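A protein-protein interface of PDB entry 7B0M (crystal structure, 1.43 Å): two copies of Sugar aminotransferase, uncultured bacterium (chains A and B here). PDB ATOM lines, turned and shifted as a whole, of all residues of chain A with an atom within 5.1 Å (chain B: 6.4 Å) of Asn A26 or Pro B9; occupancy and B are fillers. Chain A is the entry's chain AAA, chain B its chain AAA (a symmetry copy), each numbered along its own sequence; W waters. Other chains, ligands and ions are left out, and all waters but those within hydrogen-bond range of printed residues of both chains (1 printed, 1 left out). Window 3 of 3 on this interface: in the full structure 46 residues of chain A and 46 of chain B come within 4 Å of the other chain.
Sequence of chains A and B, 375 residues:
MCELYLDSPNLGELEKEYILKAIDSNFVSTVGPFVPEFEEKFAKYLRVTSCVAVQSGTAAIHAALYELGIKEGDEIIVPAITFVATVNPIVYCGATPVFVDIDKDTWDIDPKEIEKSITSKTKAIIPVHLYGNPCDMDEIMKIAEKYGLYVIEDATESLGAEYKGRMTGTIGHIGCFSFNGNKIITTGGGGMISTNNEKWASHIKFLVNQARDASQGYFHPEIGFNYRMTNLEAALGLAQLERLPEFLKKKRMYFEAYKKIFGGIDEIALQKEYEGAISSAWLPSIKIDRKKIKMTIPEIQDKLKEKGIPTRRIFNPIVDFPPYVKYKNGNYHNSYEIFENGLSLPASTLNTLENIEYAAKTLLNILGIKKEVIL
OD1 of Asn A26 touches CD1 of Leu B11 (3.9 Å).
Val A28 touches Leu B11 (CG1 to CD1, 3.7 Å).
Hydrophobic or aromatic side chains of chain A within 4 Å of the printed part of chain B: Val A28.
Printed residues of chain B that touch a printed residue of chain A: Pro B9 and Leu B11.
Hydrophobic or aromatic side chains of chain B that line the printed part of chain A: Pro B9 and Leu B11.
Among the printed residues, 3 pairs touch across the chains.
No position is printed for both chains.
Water W1 lies within hydrogen-bond range of the side-chain amide oxygen (OD1) of Asn A26, the backbone NH (N) of Leu B11 and the backbone carbonyl oxygen (O) of Pro B9.
Printed residues of chain B within 4 Å of Asn A26: Pro B9 (2.9 Å) and Leu B11 (3.9 Å).
Of the printed residues of chain B, Val A28 touches Leu B11.
Pro B9 touches just one residue of chain A: Asn A26.
Of the printed residues of chain A, Leu B11 touches Asn A26 (3.9 Å) and Val A28 (3.7 Å).
The nearest residue of chain A that does not touch Pro B9 is Val A28 (4.7 Å).
The side-chain amide nitrogen (ND2) of Asn A26 sits at hydrogen-bond distance from the backbone carbonyl oxygen (O) of Pro B9, 2.9 Å away.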
ATOM      1  N   LYS A  21       8.299   6.462   2.095  1.00  0.00           N
ATOM      2  CA  LYS A  21       9.100   6.917   0.925  1.00  0.00           C
ATOM      3  C   LYS A  21      10.588   6.713   1.224  1.00  0.00           C
ATOM      4  O   LYS A  21      11.370   6.302   0.340  1.00  0.00           O
ATOM      5  CB  LYS A  21       8.724   8.377   0.635  1.00  0.00           C
ATOM      6  CG  LYS A  21       8.881   8.890  -0.785  1.00  0.00           C
ATOM      7  CD  LYS A  21       8.612  10.402  -0.914  1.00  0.00           C
ATOM      8  CE  LYS A  21       7.217  10.839  -0.484  1.00  0.00           C
ATOM      9  NZ  LYS A  21       6.986  12.304  -0.639  1.00  0.00           N
ATOM     10  N   ALA A  22      11.043   7.038   2.441  1.00  0.00           N
ATOM     11  CA  ALA A  22      12.448   6.795   2.811  1.00  0.00           C
ATOM     12  C   ALA A  22      12.807   5.298   2.786  1.00  0.00           C
ATOM     13  O   ALA A  22      13.937   4.952   2.391  1.00  0.00           O
ATOM     14  CB  ALA A  22      12.692   7.382   4.185  1.00  0.00           C
ATOM     15  N   ILE A  23      12.004   4.456   3.399  1.00  0.00           N
ATOM     16  CA  ILE A  23      12.287   2.993   3.467  1.00  0.00           C
ATOM     17  C   ILE A  23      12.310   2.486   2.027  1.00  0.00           C
ATOM     18  O   ILE A  23      13.268   1.756   1.649  1.00  0.00           O
ATOM     19  CB  ILE A  23      11.241   2.273   4.321  1.00  0.00           C
ATOM     20  CG1 ILE A  23      11.390   2.738   5.777  1.00  0.00           C
ATOM     21  CG2 ILE A  23      11.339   0.758   4.212  1.00  0.00           C
ATOM     22  CD1 ILE A  23      10.159   2.494   6.617  1.00  0.00           C
ATOM     23  N   ASP A  24      11.325   2.896   1.235  1.00  0.00           N
ATOM     24  CA  ASP A  24      11.235   2.416  -0.191  1.00  0.00           C
ATOM     25  C   ASP A  24      12.398   2.900  -1.056  1.00  0.00           C
ATOM     26  O   ASP A  24      12.719   2.256  -2.055  1.00  0.00           O
ATOM     27  CB  ASP A  24       9.937   2.860  -0.867  1.00  0.00           C
ATOM     28  CG  ASP A  24       8.735   2.083  -0.404  1.00  0.00           C
ATOM     29  OD1 ASP A  24       8.933   0.938   0.000  1.00  0.00           O
ATOM     30  OD2 ASP A  24       7.616   2.648  -0.429  1.00  0.00           O
ATOM     31  N   SER A  25      13.038   4.014  -0.735  1.00  0.00           N
ATOM     32  CA  SER A  25      14.112   4.616  -1.537  1.00  0.00           C
ATOM     33  C   SER A  25      15.445   4.053  -1.063  1.00  0.00           C
ATOM     34  O   SER A  25      16.470   4.339  -1.688  1.00  0.00           O
ATOM     35  CB  SER A  25      14.069   6.112  -1.437  1.00  0.00           C
ATOM     36  OG  SER A  25      14.572   6.505  -0.157  1.00  0.00           O
ATOM     37  N   ASN A  26      15.404   3.374   0.093  1.00  0.00           N
ATOM     38  CA  ASN A  26      16.571   2.799   0.808  1.00  0.00           C
ATOM     39  C   ASN A  26      17.393   3.882   1.521  1.00  0.00           C
ATOM     40  O   ASN A  26      18.441   3.567   2.080  1.00  0.00           O
ATOM     41  CB  ASN A  26      17.436   2.005  -0.161  1.00  0.00           C
ATOM     42  CG  ASN A  26      17.582   0.588   0.309  1.00  0.00           C
ATOM     43  OD1 ASN A  26      16.581  -0.031   0.676  1.00  0.00           O
ATOM     44  ND2 ASN A  26      18.814   0.098   0.302  1.00  0.00           N
ATOM     45  N   PHE A  27      16.922   5.134   1.487  1.00  0.00           N
ATOM     46  CA  PHE A  27      17.618   6.307   2.075  1.00  0.00           C
ATOM     47  C   PHE A  27      17.097   6.498   3.516  1.00  0.00           C
ATOM     48  O   PHE A  27      16.259   7.381   3.771  1.00  0.00           O
ATOM     49  CB  PHE A  27      17.395   7.525   1.173  1.00  0.00           C
ATOM     50  CG  PHE A  27      18.066   7.450  -0.182  1.00  0.00           C
ATOM     51  CD1 PHE A  27      19.431   7.200  -0.273  1.00  0.00           C
ATOM     52  CD2 PHE A  27      17.379   7.738  -1.349  1.00  0.00           C
ATOM     53  CE1 PHE A  27      20.105   7.171  -1.491  1.00  0.00           C
ATOM     54  CE2 PHE A  27      18.055   7.727  -2.570  1.00  0.00           C
ATOM     55  CZ  PHE A  27      19.410   7.454  -2.634  1.00  0.00           C
ATOM     56  N   VAL A  28      17.671   5.738   4.449  1.00  0.00           N
ATOM     57  CA  VAL A  28      17.256   5.824   5.868  1.00  0.00           C
ATOM     58  C   VAL A  28      18.430   6.336   6.723  1.00  0.00           C
ATOM     59  O   VAL A  28      18.188   6.658   7.943  1.00  0.00           O
ATOM     60  CB  VAL A  28      16.681   4.484   6.384  1.00  0.00           C
ATOM     61  CG1 VAL A  28      15.410   4.090   5.624  1.00  0.00           C
ATOM     62  CG2 VAL A  28      17.710   3.342   6.360  1.00  0.00           C
ATOM     63  N   ASP B   7      27.438  -2.115   0.135  1.00  0.00           N
ATOM     64  CA  ASP B   7      27.064  -2.207   1.567  1.00  0.00           C
ATOM     65  C   ASP B   7      25.675  -1.625   1.847  1.00  0.00           C
ATOM     66  O   ASP B   7      25.384  -1.321   2.993  1.00  0.00           O
ATOM     67  CB  ASP B   7      28.111  -1.494   2.415  1.00  0.00           C
ATOM     68  CG  ASP B   7      28.267  -0.033   2.004  1.00  0.00           C
ATOM     69  OD1 ASP B   7      27.456   0.461   1.228  1.00  0.00           O
ATOM     70  OD2 ASP B   7      29.258   0.585   2.432  1.00  0.00           O
ATOM     71  N   SER B   8      24.808  -1.563   0.853  1.00  0.00           N
ATOM     72  CA  SER B   8      23.459  -0.978   0.977  1.00  0.00           C
ATOM     73  C   SER B   8      22.651  -1.786   1.974  1.00  0.00           C
ATOM     74  O   SER B   8      22.788  -3.014   2.042  1.00  0.00           O
ATOM     75  CB  SER B   8      22.755  -0.949  -0.340  1.00  0.00           C
ATOM     76  OG  SER B   8      23.486  -0.177  -1.270  1.00  0.00           O
ATOM     77  N   PRO B   9      21.764  -1.117   2.735  1.00  0.00           N
ATOM     78  CA  PRO B   9      20.879  -1.814   3.659  1.00  0.00           C
ATOM     79  C   PRO B   9      19.810  -2.579   2.864  1.00  0.00           C
ATOM     80  O   PRO B   9      19.625  -2.302   1.682  1.00  0.00           O
ATOM     81  CB  PRO B   9      20.312  -0.700   4.537  1.00  0.00           C
ATOM     82  CG  PRO B   9      20.367   0.535   3.684  1.00  0.00           C
ATOM     83  CD  PRO B   9      21.597   0.356   2.803  1.00  0.00           C
ATOM     84  N   ASN B  10      19.180  -3.495   3.561  1.00  0.00           N
ATOM     85  CA  ASN B  10      18.211  -4.498   3.057  1.00  0.00           C
ATOM     86  C   ASN B  10      16.910  -4.299   3.825  1.00  0.00           C
ATOM     87  O   ASN B  10      16.790  -4.779   4.926  1.00  0.00           O
ATOM     88  CB  ASN B  10      18.799  -5.898   3.226  1.00  0.00           C
ATOM     89  CG  ASN B  10      17.943  -6.957   2.574  1.00  0.00           C
ATOM     90  OD1 ASN B  10      16.728  -6.821   2.527  1.00  0.00           O
ATOM     91  ND2 ASN B  10      18.558  -8.070   2.237  1.00  0.00           N
ATOM     92  N   LEU B  11      16.003  -3.511   3.291  1.00  0.00           N
ATOM     93  CA  LEU B  11      14.750  -3.079   3.942  1.00  0.00           C
ATOM     94  C   LEU B  11      13.573  -3.540   3.083  1.00  0.00           C
ATOM     95  O   LEU B  11      13.583  -3.282   1.890  1.00  0.00           O
ATOM     96  CB  LEU B  11      14.741  -1.554   4.008  1.00  0.00           C
ATOM     97  CG  LEU B  11      16.005  -0.922   4.593  1.00  0.00           C
ATOM     98  CD1 LEU B  11      15.965   0.599   4.477  1.00  0.00           C
ATOM     99  CD2 LEU B  11      16.213  -1.296   6.050  1.00  0.00           C
ATOM    100  N   ASN B 180      24.571   1.816  11.859  1.00  0.00           N
ATOM    101  CA  ASN B 180      24.632   2.776  10.745  1.00  0.00           C
ATOM    102  C   ASN B 180      24.207   2.053   9.431  1.00  0.00           C
ATOM    103  O   ASN B 180      24.135   0.787   9.422  1.00  0.00           O
ATOM    104  CB  ASN B 180      26.012   3.411  10.627  1.00  0.00           C
ATOM    105  CG  ASN B 180      25.941   4.846  10.131  1.00  0.00           C
ATOM    106  OD1 ASN B 180      25.047   5.205   9.381  1.00  0.00           O
ATOM    107  ND2 ASN B 180      26.894   5.648  10.528  1.00  0.00           N
ATOM    108  N   GLY B 181      23.869   2.767   8.393  1.00  0.00           N
ATOM    109  CA  GLY B 181      23.190   2.261   7.188  1.00  0.00           C
ATOM    110  C   GLY B 181      23.934   1.108   6.520  1.00  0.00           C
ATOM    111  O   GLY B 181      23.213   0.228   5.951  1.00  0.00           O
ATOM    112  N   ASN B 182      25.260   1.101   6.572  1.00  0.00           N
ATOM    113  CA  ASN B 182      26.063   0.108   5.836  1.00  0.00           C
ATOM    114  C   ASN B 182      26.381  -1.098   6.720  1.00  0.00           C
ATOM    115  O   ASN B 182      27.123  -1.961   6.248  1.00  0.00           O
ATOM    116  CB  ASN B 182      27.395   0.726   5.392  1.00  0.00           C
ATOM    117  CG  ASN B 182      28.218   1.391   6.479  1.00  0.00           C
ATOM    118  OD1 ASN B 182      27.713   1.844   7.516  1.00  0.00           O
ATOM    119  ND2 ASN B 182      29.511   1.591   6.209  1.00  0.00           N
ATOM    120  N1  LLP B 183      34.115   1.900  14.712  1.00  0.00           N
ATOM    121  C2  LLP B 183      34.151   1.253  13.542  1.00  0.00           C
ATOM    122  C2' LLP B 183      35.313   0.335  13.340  1.00  0.00           C
ATOM    123  C3  LLP B 183      33.199   1.433  12.574  1.00  0.00           C
ATOM    124  O3  LLP B 183      33.202   0.782  11.403  1.00  0.00           O
ATOM    125  C4  LLP B 183      32.116   2.316  12.830  1.00  0.00           C
ATOM    126  C4' LLP B 183      30.992   2.337  11.858  1.00  0.00           C
ATOM    127  C5  LLP B 183      32.170   3.040  14.049  1.00  0.00           C
ATOM    128  C6  LLP B 183      33.153   2.824  14.938  1.00  0.00           C
ATOM    129  C5' LLP B 183      31.192   4.150  14.308  1.00  0.00           C
ATOM    130  OP4 LLP B 183      29.799   3.794  14.341  1.00  0.00           O
ATOM    131  P   LLP B 183      28.689   4.894  13.924  1.00  0.00           P
ATOM    132  OP1 LLP B 183      28.848   6.113  14.856  1.00  0.00           O
ATOM    133  OP2 LLP B 183      28.879   5.207  12.455  1.00  0.00           O
ATOM    134  OP3 LLP B 183      27.393   4.158  14.199  1.00  0.00           O
ATOM    135  N   LLP B 183      26.017  -1.112   8.006  1.00  0.00           N
ATOM    136  CA  LLP B 183      26.423  -2.201   8.889  1.00  0.00           C
ATOM    137  CB  LLP B 183      26.358  -1.734  10.363  1.00  0.00           C
ATOM    138  CG  LLP B 183      27.184  -0.475  10.641  1.00  0.00           C
ATOM    139  CD  LLP B 183      28.710  -0.518  10.598  1.00  0.00           C
ATOM    140  CE  LLP B 183      29.289   0.963  10.634  1.00  0.00           C
ATOM    141  NZ  LLP B 183      30.614   1.177  11.219  1.00  0.00           N
ATOM    142  C   LLP B 183      25.533  -3.424   8.619  1.00  0.00           C
ATOM    143  O   LLP B 183      24.609  -3.365   7.811  1.00  0.00           O
ATOM    144  N   THR B 186      20.679  -2.239  10.301  1.00  0.00           N
ATOM    145  CA  THR B 186      20.622  -0.759  10.482  1.00  0.00           C
ATOM    146  C   THR B 186      19.354  -0.325  11.186  1.00  0.00           C
ATOM    147  O   THR B 186      18.245  -0.904  11.039  1.00  0.00           O
ATOM    148  CB  THR B 186      20.790  -0.027   9.153  1.00  0.00           C
ATOM    149  OG1 THR B 186      20.923   1.390   9.371  1.00  0.00           O
ATOM    150  CG2 THR B 186      19.584  -0.245   8.256  1.00  0.00           C
ATOM    151  N   GLN B 240      15.058  -5.693  11.731  1.00  0.00           N
ATOM    152  CA  GLN B 240      16.348  -6.148  11.200  1.00  0.00           C
ATOM    153  C   GLN B 240      16.906  -7.300  12.040  1.00  0.00           C
ATOM    154  O   GLN B 240      17.528  -8.195  11.428  1.00  0.00           O
ATOM    155  CB  GLN B 240      17.332  -4.983  11.183  1.00  0.00           C
ATOM    156  CG  GLN B 240      16.972  -3.905  10.151  1.00  0.00           C
ATOM    157  CD  GLN B 240      17.691  -4.129   8.858  1.00  0.00           C
ATOM    158  OE1 GLN B 240      18.899  -3.897   8.722  1.00  0.00           O
ATOM    159  NE2 GLN B 240      16.957  -4.602   7.876  1.00  0.00           N
ATOM    160  N   SER B 348      26.876  -6.289   0.372  1.00  0.00           N
ATOM    161  CA  SER B 348      25.481  -5.996   0.764  1.00  0.00           C
ATOM    162  C   SER B 348      24.671  -7.295   0.716  1.00  0.00           C
ATOM    163  O   SER B 348      24.840  -8.071  -0.240  1.00  0.00           O
ATOM    164  CB  SER B 348      24.862  -4.964  -0.093  1.00  0.00           C
ATOM    165  OG  SER B 348      23.446  -4.871   0.150  1.00  0.00           O
ATOM    166  N   THR B 349      23.790  -7.509   1.683  1.00  0.00           N
ATOM    167  CA  THR B 349      22.882  -8.684   1.715  1.00  0.00           C
ATOM    168  C   THR B 349      21.852  -8.582   0.574  1.00  0.00           C
ATOM    169  O   THR B 349      21.080  -9.543   0.466  1.00  0.00           O
ATOM    170  CB  THR B 349      22.216  -8.865   3.064  1.00  0.00           C
ATOM    171  OG1 THR B 349      21.426  -7.710   3.319  1.00  0.00           O
ATOM    172  CG2 THR B 349      23.226  -9.084   4.161  1.00  0.00           C
ATOM    173  N   LEU B 350      21.764  -7.459  -0.168  1.00  0.00           N
ATOM    174  CA  LEU B 350      20.982  -7.399  -1.449  1.00  0.00           C
ATOM    175  C   LEU B 350      21.610  -8.275  -2.535  1.00  0.00           C
ATOM    176  O   LEU B 350      20.917  -8.542  -3.520  1.00  0.00           O
ATOM    177  CB  LEU B 350      20.871  -5.955  -1.916  1.00  0.00           C
ATOM    178  CG  LEU B 350      20.075  -5.042  -0.997  1.00  0.00           C
ATOM    179  CD1 LEU B 350      19.984  -3.645  -1.613  1.00  0.00           C
ATOM    180  CD2 LEU B 350      18.654  -5.574  -0.751  1.00  0.00           C
HETATM  181  O   HOH W   1      16.745  -2.441   0.671  1.00  0.00           O
